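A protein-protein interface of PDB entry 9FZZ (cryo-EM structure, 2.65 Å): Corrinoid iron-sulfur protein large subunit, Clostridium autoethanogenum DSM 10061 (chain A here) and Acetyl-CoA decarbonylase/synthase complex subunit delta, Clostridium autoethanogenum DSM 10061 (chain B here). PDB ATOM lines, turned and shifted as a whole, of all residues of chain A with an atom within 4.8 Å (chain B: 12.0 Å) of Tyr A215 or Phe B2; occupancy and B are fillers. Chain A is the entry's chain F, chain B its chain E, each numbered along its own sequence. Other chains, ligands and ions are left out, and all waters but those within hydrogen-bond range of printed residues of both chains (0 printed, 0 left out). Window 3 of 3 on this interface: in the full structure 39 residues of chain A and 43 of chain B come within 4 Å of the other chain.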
ATOM      1  N   LEU A 211     -27.788  13.203 -14.628  1.00  0.00           N
ATOM      2  CA  LEU A 211     -27.147  12.571 -13.480  1.00  0.00           C
ATOM      3  C   LEU A 211     -25.701  12.207 -13.774  1.00  0.00           C
ATOM      4  O   LEU A 211     -24.842  12.324 -12.898  1.00  0.00           O
ATOM      5  CB  LEU A 211     -27.928  11.334 -13.040  1.00  0.00           C
ATOM      6  CG  LEU A 211     -29.245  11.631 -12.307  1.00  0.00           C
ATOM      7  CD1 LEU A 211     -29.775  10.363 -11.677  1.00  0.00           C
ATOM      8  CD2 LEU A 211     -29.081  12.708 -11.239  1.00  0.00           C
ATOM      9  N   GLU A 212     -25.407  11.745 -14.988  1.00  0.00           N
ATOM     10  CA  GLU A 212     -24.030  11.386 -15.318  1.00  0.00           C
ATOM     11  C   GLU A 212     -23.124  12.611 -15.317  1.00  0.00           C
ATOM     12  O   GLU A 212     -22.009  12.577 -14.779  1.00  0.00           O
ATOM     13  CB  GLU A 212     -23.981  10.688 -16.673  1.00  0.00           C
ATOM     14  CG  GLU A 212     -24.145   9.181 -16.572  1.00  0.00           C
ATOM     15  CD  GLU A 212     -23.786   8.488 -17.870  1.00  0.00           C
ATOM     16  OE1 GLU A 212     -23.291   9.179 -18.780  1.00  0.00           O
ATOM     17  OE2 GLU A 212     -23.997   7.262 -17.981  1.00  0.00           O
ATOM     18  N   ALA A 213     -23.581  13.699 -15.929  1.00  0.00           N
ATOM     19  CA  ALA A 213     -22.790  14.925 -15.918  1.00  0.00           C
ATOM     20  C   ALA A 213     -22.636  15.467 -14.504  1.00  0.00           C
ATOM     21  O   ALA A 213     -21.552  15.918 -14.119  1.00  0.00           O
ATOM     22  CB  ALA A 213     -23.431  15.967 -16.838  1.00  0.00           C
ATOM     23  N   LEU A 214     -23.706  15.416 -13.710  1.00  0.00           N
ATOM     24  CA  LEU A 214     -23.612  15.855 -12.322  1.00  0.00           C
ATOM     25  C   LEU A 214     -22.618  15.007 -11.541  1.00  0.00           C
ATOM     26  O   LEU A 214     -21.828  15.532 -10.749  1.00  0.00           O
ATOM     27  CB  LEU A 214     -24.994  15.810 -11.662  1.00  0.00           C
ATOM     28  CG  LEU A 214     -25.057  16.321 -10.214  1.00  0.00           C
ATOM     29  CD1 LEU A 214     -24.641  17.786 -10.124  1.00  0.00           C
ATOM     30  CD2 LEU A 214     -26.457  16.130  -9.660  1.00  0.00           C
ATOM     31  N   TYR A 215     -22.635  13.694 -11.762  1.00  0.00           N
ATOM     32  CA  TYR A 215     -21.708  12.800 -11.078  1.00  0.00           C
ATOM     33  C   TYR A 215     -20.265  13.108 -11.452  1.00  0.00           C
ATOM     34  O   TYR A 215     -19.384  13.146 -10.586  1.00  0.00           O
ATOM     35  CB  TYR A 215     -22.062  11.352 -11.425  1.00  0.00           C
ATOM     36  CG  TYR A 215     -21.462  10.331 -10.500  1.00  0.00           C
ATOM     37  CD1 TYR A 215     -20.184   9.815 -10.728  1.00  0.00           C
ATOM     38  CD2 TYR A 215     -22.173   9.872  -9.389  1.00  0.00           C
ATOM     39  CE1 TYR A 215     -19.624   8.868  -9.869  1.00  0.00           C
ATOM     40  CE2 TYR A 215     -21.631   8.927  -8.523  1.00  0.00           C
ATOM     41  CZ  TYR A 215     -20.357   8.435  -8.772  1.00  0.00           C
ATOM     42  OH  TYR A 215     -19.827   7.498  -7.909  1.00  0.00           O
ATOM     43  N   GLY A 216     -20.008  13.340 -12.739  1.00  0.00           N
ATOM     44  CA  GLY A 216     -18.664  13.702 -13.162  1.00  0.00           C
ATOM     45  C   GLY A 216     -18.200  15.020 -12.571  1.00  0.00           C
ATOM     46  O   GLY A 216     -17.055  15.146 -12.123  1.00  0.00           O
ATOM     47  N   LEU A 217     -19.086  16.015 -12.549  1.00  0.00           N
ATOM     48  CA  LEU A 217     -18.735  17.311 -11.975  1.00  0.00           C
ATOM     49  C   LEU A 217     -18.441  17.196 -10.486  1.00  0.00           C
ATOM     50  O   LEU A 217     -17.492  17.810  -9.985  1.00  0.00           O
ATOM     51  CB  LEU A 217     -19.862  18.314 -12.228  1.00  0.00           C
ATOM     52  CG  LEU A 217     -19.620  19.737 -11.711  1.00  0.00           C
ATOM     53  CD1 LEU A 217     -18.298  20.288 -12.221  1.00  0.00           C
ATOM     54  CD2 LEU A 217     -20.767  20.629 -12.146  1.00  0.00           C
ATOM     55  N   VAL A 218     -19.233  16.406  -9.762  1.00  0.00           N
ATOM     56  CA  VAL A 218     -18.990  16.226  -8.333  1.00  0.00           C
ATOM     57  C   VAL A 218     -17.685  15.478  -8.105  1.00  0.00           C
ATOM     58  O   VAL A 218     -16.949  15.764  -7.156  1.00  0.00           O
ATOM     59  CB  VAL A 218     -20.178  15.519  -7.669  1.00  0.00           C
ATOM     60  CG1 VAL A 218     -19.871  15.222  -6.209  1.00  0.00           C
ATOM     61  CG2 VAL A 218     -21.420  16.391  -7.765  1.00  0.00           C
ATOM     62  N   GLU A 219     -17.372  14.507  -8.964  1.00  0.00           N
ATOM     63  CA  GLU A 219     -16.083  13.824  -8.851  1.00  0.00           C
ATOM     64  C   GLU A 219     -14.926  14.796  -9.047  1.00  0.00           C
ATOM     65  O   GLU A 219     -13.936  14.754  -8.309  1.00  0.00           O
ATOM     66  CB  GLU A 219     -15.994  12.683  -9.861  1.00  0.00           C
ATOM     67  CG  GLU A 219     -16.699  11.417  -9.395  1.00  0.00           C
ATOM     68  CD  GLU A 219     -16.500  10.267 -10.363  1.00  0.00           C
ATOM     69  OE1 GLU A 219     -16.337  10.536 -11.569  1.00  0.00           O
ATOM     70  OE2 GLU A 219     -16.490   9.100  -9.919  1.00  0.00           O
ATOM     71  N   ILE A 251     -28.935   6.181  -5.136  1.00  0.00           N
ATOM     72  CA  ILE A 251     -27.519   5.901  -5.368  1.00  0.00           C
ATOM     73  C   ILE A 251     -26.720   6.149  -4.102  1.00  0.00           C
ATOM     74  O   ILE A 251     -25.833   5.367  -3.746  1.00  0.00           O
ATOM     75  CB  ILE A 251     -26.991   6.744  -6.538  1.00  0.00           C
ATOM     76  CG1 ILE A 251     -27.570   6.235  -7.856  1.00  0.00           C
ATOM     77  CG2 ILE A 251     -25.466   6.705  -6.588  1.00  0.00           C
ATOM     78  CD1 ILE A 251     -27.416   7.216  -8.999  1.00  0.00           C
ATOM     79  N   ASP A 257     -22.858   4.981  -2.206  1.00  0.00           N
ATOM     80  CA  ASP A 257     -21.937   5.820  -2.960  1.00  0.00           C
ATOM     81  C   ASP A 257     -21.967   7.221  -2.368  1.00  0.00           C
ATOM     82  O   ASP A 257     -23.022   7.864  -2.340  1.00  0.00           O
ATOM     83  CB  ASP A 257     -22.327   5.840  -4.434  1.00  0.00           C
ATOM     84  CG  ASP A 257     -21.224   6.358  -5.322  1.00  0.00           C
ATOM     85  OD1 ASP A 257     -20.165   6.734  -4.782  1.00  0.00           O
ATOM     86  OD2 ASP A 257     -21.406   6.389  -6.553  1.00  0.00           O
ATOM     87  N   THR A 259     -20.428   9.898  -3.514  1.00  0.00           N
ATOM     88  CA  THR A 259     -20.368  10.990  -4.477  1.00  0.00           C
ATOM     89  C   THR A 259     -21.691  11.741  -4.526  1.00  0.00           C
ATOM     90  O   THR A 259     -21.710  12.965  -4.679  1.00  0.00           O
ATOM     91  CB  THR A 259     -20.003  10.452  -5.857  1.00  0.00           C
ATOM     92  OG1 THR A 259     -18.803   9.672  -5.780  1.00  0.00           O
ATOM     93  CG2 THR A 259     -19.780  11.592  -6.827  1.00  0.00           C
ATOM     94  N   PHE A 260     -22.809  11.028  -4.400  1.00  0.00           N
ATOM     95  CA  PHE A 260     -24.123  11.643  -4.317  1.00  0.00           C
ATOM     96  C   PHE A 260     -24.610  11.804  -2.881  1.00  0.00           C
ATOM     97  O   PHE A 260     -25.813  11.939  -2.649  1.00  0.00           O
ATOM     98  CB  PHE A 260     -25.138  10.837  -5.136  1.00  0.00           C
ATOM     99  CG  PHE A 260     -25.142  11.154  -6.618  1.00  0.00           C
ATOM    100  CD1 PHE A 260     -24.558  12.327  -7.111  1.00  0.00           C
ATOM    101  CD2 PHE A 260     -25.740  10.282  -7.517  1.00  0.00           C
ATOM    102  CE1 PHE A 260     -24.565  12.620  -8.475  1.00  0.00           C
ATOM    103  CE2 PHE A 260     -25.757  10.557  -8.889  1.00  0.00           C
ATOM    104  CZ  PHE A 260     -25.166  11.733  -9.368  1.00  0.00           C
ATOM    105  N   PHE B   2     -20.939   5.064 -11.804  1.00  0.00           N
ATOM    106  CA  PHE B   2     -21.955   4.701 -10.829  1.00  0.00           C
ATOM    107  C   PHE B   2     -22.948   3.767 -11.509  1.00  0.00           C
ATOM    108  O   PHE B   2     -23.110   3.786 -12.731  1.00  0.00           O
ATOM    109  CB  PHE B   2     -22.669   5.928 -10.236  1.00  0.00           C
ATOM    110  CG  PHE B   2     -23.568   6.652 -11.201  1.00  0.00           C
ATOM    111  CD1 PHE B   2     -23.047   7.606 -12.071  1.00  0.00           C
ATOM    112  CD2 PHE B   2     -24.936   6.388 -11.231  1.00  0.00           C
ATOM    113  CE1 PHE B   2     -23.872   8.286 -12.975  1.00  0.00           C
ATOM    114  CE2 PHE B   2     -25.783   7.057 -12.127  1.00  0.00           C
ATOM    115  CZ  PHE B   2     -25.248   8.011 -13.004  1.00  0.00           C
ATOM    116  N   LYS B   3     -23.612   2.949 -10.701  1.00  0.00           N
ATOM    117  CA  LYS B   3     -24.584   1.976 -11.179  1.00  0.00           C
ATOM    118  C   LYS B   3     -25.983   2.526 -10.938  1.00  0.00           C
ATOM    119  O   LYS B   3     -26.283   3.026  -9.850  1.00  0.00           O
ATOM    120  CB  LYS B   3     -24.423   0.627 -10.476  1.00  0.00           C
ATOM    121  CG  LYS B   3     -23.440  -0.326 -11.180  1.00  0.00           C
ATOM    122  CD  LYS B   3     -21.996   0.201 -11.095  1.00  0.00           C
ATOM    123  CE  LYS B   3     -21.178  -0.220 -12.323  1.00  0.00           C
ATOM    124  NZ  LYS B   3     -19.894   0.557 -12.409  1.00  0.00           N
ATOM    125  N   LYS B   4     -26.825   2.442 -11.962  1.00  0.00           N
ATOM    126  CA  LYS B   4     -28.192   2.911 -11.836  1.00  0.00           C
ATOM    127  C   LYS B   4     -28.931   2.056 -10.812  1.00  0.00           C
ATOM    128  O   LYS B   4     -28.742   0.832 -10.773  1.00  0.00           O
ATOM    129  CB  LYS B   4     -28.904   2.840 -13.188  1.00  0.00           C
ATOM    130  CG  LYS B   4     -30.019   3.880 -13.360  1.00  0.00           C
ATOM    131  CD  LYS B   4     -29.423   5.294 -13.474  1.00  0.00           C
ATOM    132  CE  LYS B   4     -30.499   6.309 -13.860  1.00  0.00           C
ATOM    133  NZ  LYS B   4     -29.935   7.680 -14.069  1.00  0.00           N
ATOM    134  N   PRO B   5     -29.770   2.661  -9.949  1.00  0.00           N
ATOM    135  CA  PRO B   5     -30.498   1.848  -8.962  1.00  0.00           C
ATOM    136  C   PRO B   5     -31.559   0.980  -9.620  1.00  0.00           C
ATOM    137  O   PRO B   5     -32.598   1.484 -10.065  1.00  0.00           O
ATOM    138  CB  PRO B   5     -31.118   2.890  -8.016  1.00  0.00           C
ATOM    139  CG  PRO B   5     -30.343   4.173  -8.262  1.00  0.00           C
ATOM    140  CD  PRO B   5     -29.947   4.108  -9.713  1.00  0.00           C
ATOM    141  N   THR B   6     -31.304  -0.329  -9.691  1.00  0.00           N
ATOM    142  CA  THR B   6     -32.231  -1.288 -10.284  1.00  0.00           C
ATOM    143  C   THR B   6     -32.930  -2.005  -9.134  1.00  0.00           C
ATOM    144  O   THR B   6     -32.408  -2.979  -8.586  1.00  0.00           O
ATOM    145  CB  THR B   6     -31.507  -2.280 -11.188  1.00  0.00           C
ATOM    146  OG1 THR B   6     -30.772  -1.583 -12.203  1.00  0.00           O
ATOM    147  CG2 THR B   6     -32.507  -3.213 -11.857  1.00  0.00           C
ATOM    148  N   PHE B  38     -39.170   5.072 -13.930  1.00  0.00           N
ATOM    149  CA  PHE B  38     -37.801   4.728 -14.291  1.00  0.00           C
ATOM    150  C   PHE B  38     -37.368   3.377 -13.735  1.00  0.00           C
ATOM    151  O   PHE B  38     -36.247   2.947 -14.013  1.00  0.00           O
ATOM    152  CB  PHE B  38     -36.834   5.820 -13.805  1.00  0.00           C
ATOM    153  CG  PHE B  38     -37.106   6.298 -12.402  1.00  0.00           C
ATOM    154  CD1 PHE B  38     -36.529   5.659 -11.308  1.00  0.00           C
ATOM    155  CD2 PHE B  38     -37.955   7.381 -12.177  1.00  0.00           C
ATOM    156  CE1 PHE B  38     -36.790   6.090 -10.005  1.00  0.00           C
ATOM    157  CE2 PHE B  38     -38.229   7.826 -10.882  1.00  0.00           C
ATOM    158  CZ  PHE B  38     -37.642   7.179  -9.792  1.00  0.00           C
ATOM    159  N   ASP B  39     -38.222   2.706 -12.951  1.00  0.00           N
ATOM    160  CA  ASP B  39     -37.895   1.403 -12.395  1.00  0.00           C
ATOM    161  C   ASP B  39     -38.669   0.256 -13.020  1.00  0.00           C
ATOM    162  O   ASP B  39     -38.287  -0.900 -12.825  1.00  0.00           O
ATOM    163  CB  ASP B  39     -38.162   1.371 -10.884  1.00  0.00           C
ATOM    164  CG  ASP B  39     -37.031   1.952 -10.078  1.00  0.00           C
ATOM    165  OD1 ASP B  39     -36.040   2.391 -10.697  1.00  0.00           O
ATOM    166  OD2 ASP B  39     -37.121   1.969  -8.838  1.00  0.00           O
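The backbone carbonyl oxygen of Lys B4 is in hydrogen-bond range of the side-chain hydroxyl of Thr B6.
The side-chain hydroxyl (OH) of Tyr A215 lies close to the side-chain carboxylate (OD1) of Asp A257 (3.2 Å).
The side-chain hydroxyl of Tyr A215 is in hydrogen-bond range of the side-chain hydroxyl of Thr A259 (3.2 Å).
O of Ile A251 lies within hydrogen-bond range of N of Asp A257.
OG1 of Thr A259 is in hydrogen-bond range of OD1 of Asp A257.
CD1 of Leu A211 touches NZ of Lys B4, at 3.6 Å.
CE1 of Phe B2 touches CG of Glu A212 (3.7 Å).
Phe B2 touches Tyr A215 (CD1 to CG, 3.5 Å).
CD1 of Ile A251 touches CD2 of Phe B2, 3.4 Å away.
CG1 of Ile A251 touches O of Lys B3 (3.99 Å).
Ile A251 touches Pro B5 (CG1 to CG, 3.5 Å).
Phe B2 touches Asp A257.
Of chain B, only Phe B2 (3.5 Å) comes within 4 Å of Tyr A215.
Phe B2 touches four residues of chain A.
Of chain B, only Lys B4 comes within 4 Å of Leu A211.
Glu A212 touches one residue of chain B.
No residue of chain B comes within 4 Å of Ala A213.
No residue of chain B comes within 4 Å of Gly A216.
Leu A217 touches none of the printed residues of chain B.
No residue of chain B comes within 4 Å of Glu A219.
Of the printed residues of chain B, Asp A257 touches Phe B2 (3.9 Å).
No residue of chain B comes within 4 Å of Thr A259.
No residue of chain B comes within 4 Å of Phe A260.
Of the printed residues of chain A, Lys B3 touches Ile A251 (3.99 Å).
Of the printed residues of chain A, Lys B4 touches Leu A211 (3.6 Å).
Phe B38 touches none of the printed residues of chain A.
Of the 7 printed residues of chain B, 4 touch a printed residue of chain A.
Hydrophobic or aromatic side chains of chain B that line the printed part of chain A: Phe B2 and Pro B5.
Of the 13 printed residues of chain A, 5 touch a printed residue of chain B.
Printed residues of chain A that touch a printed residue of chain B: Leu A211, Glu A212, Tyr A215, Ile A251 and Asp A257.
Hydrophobic or aromatic side chains of chain A that line the printed part of chain B: Leu A211, Tyr A215 and Ile A251.
Among the printed residues, 7 pairs touch across the chains.
Among the printed residues, no Asp or Glu carboxylate lies within 4 Å of a Lys or Arg side-chain nitrogen of the other chain.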
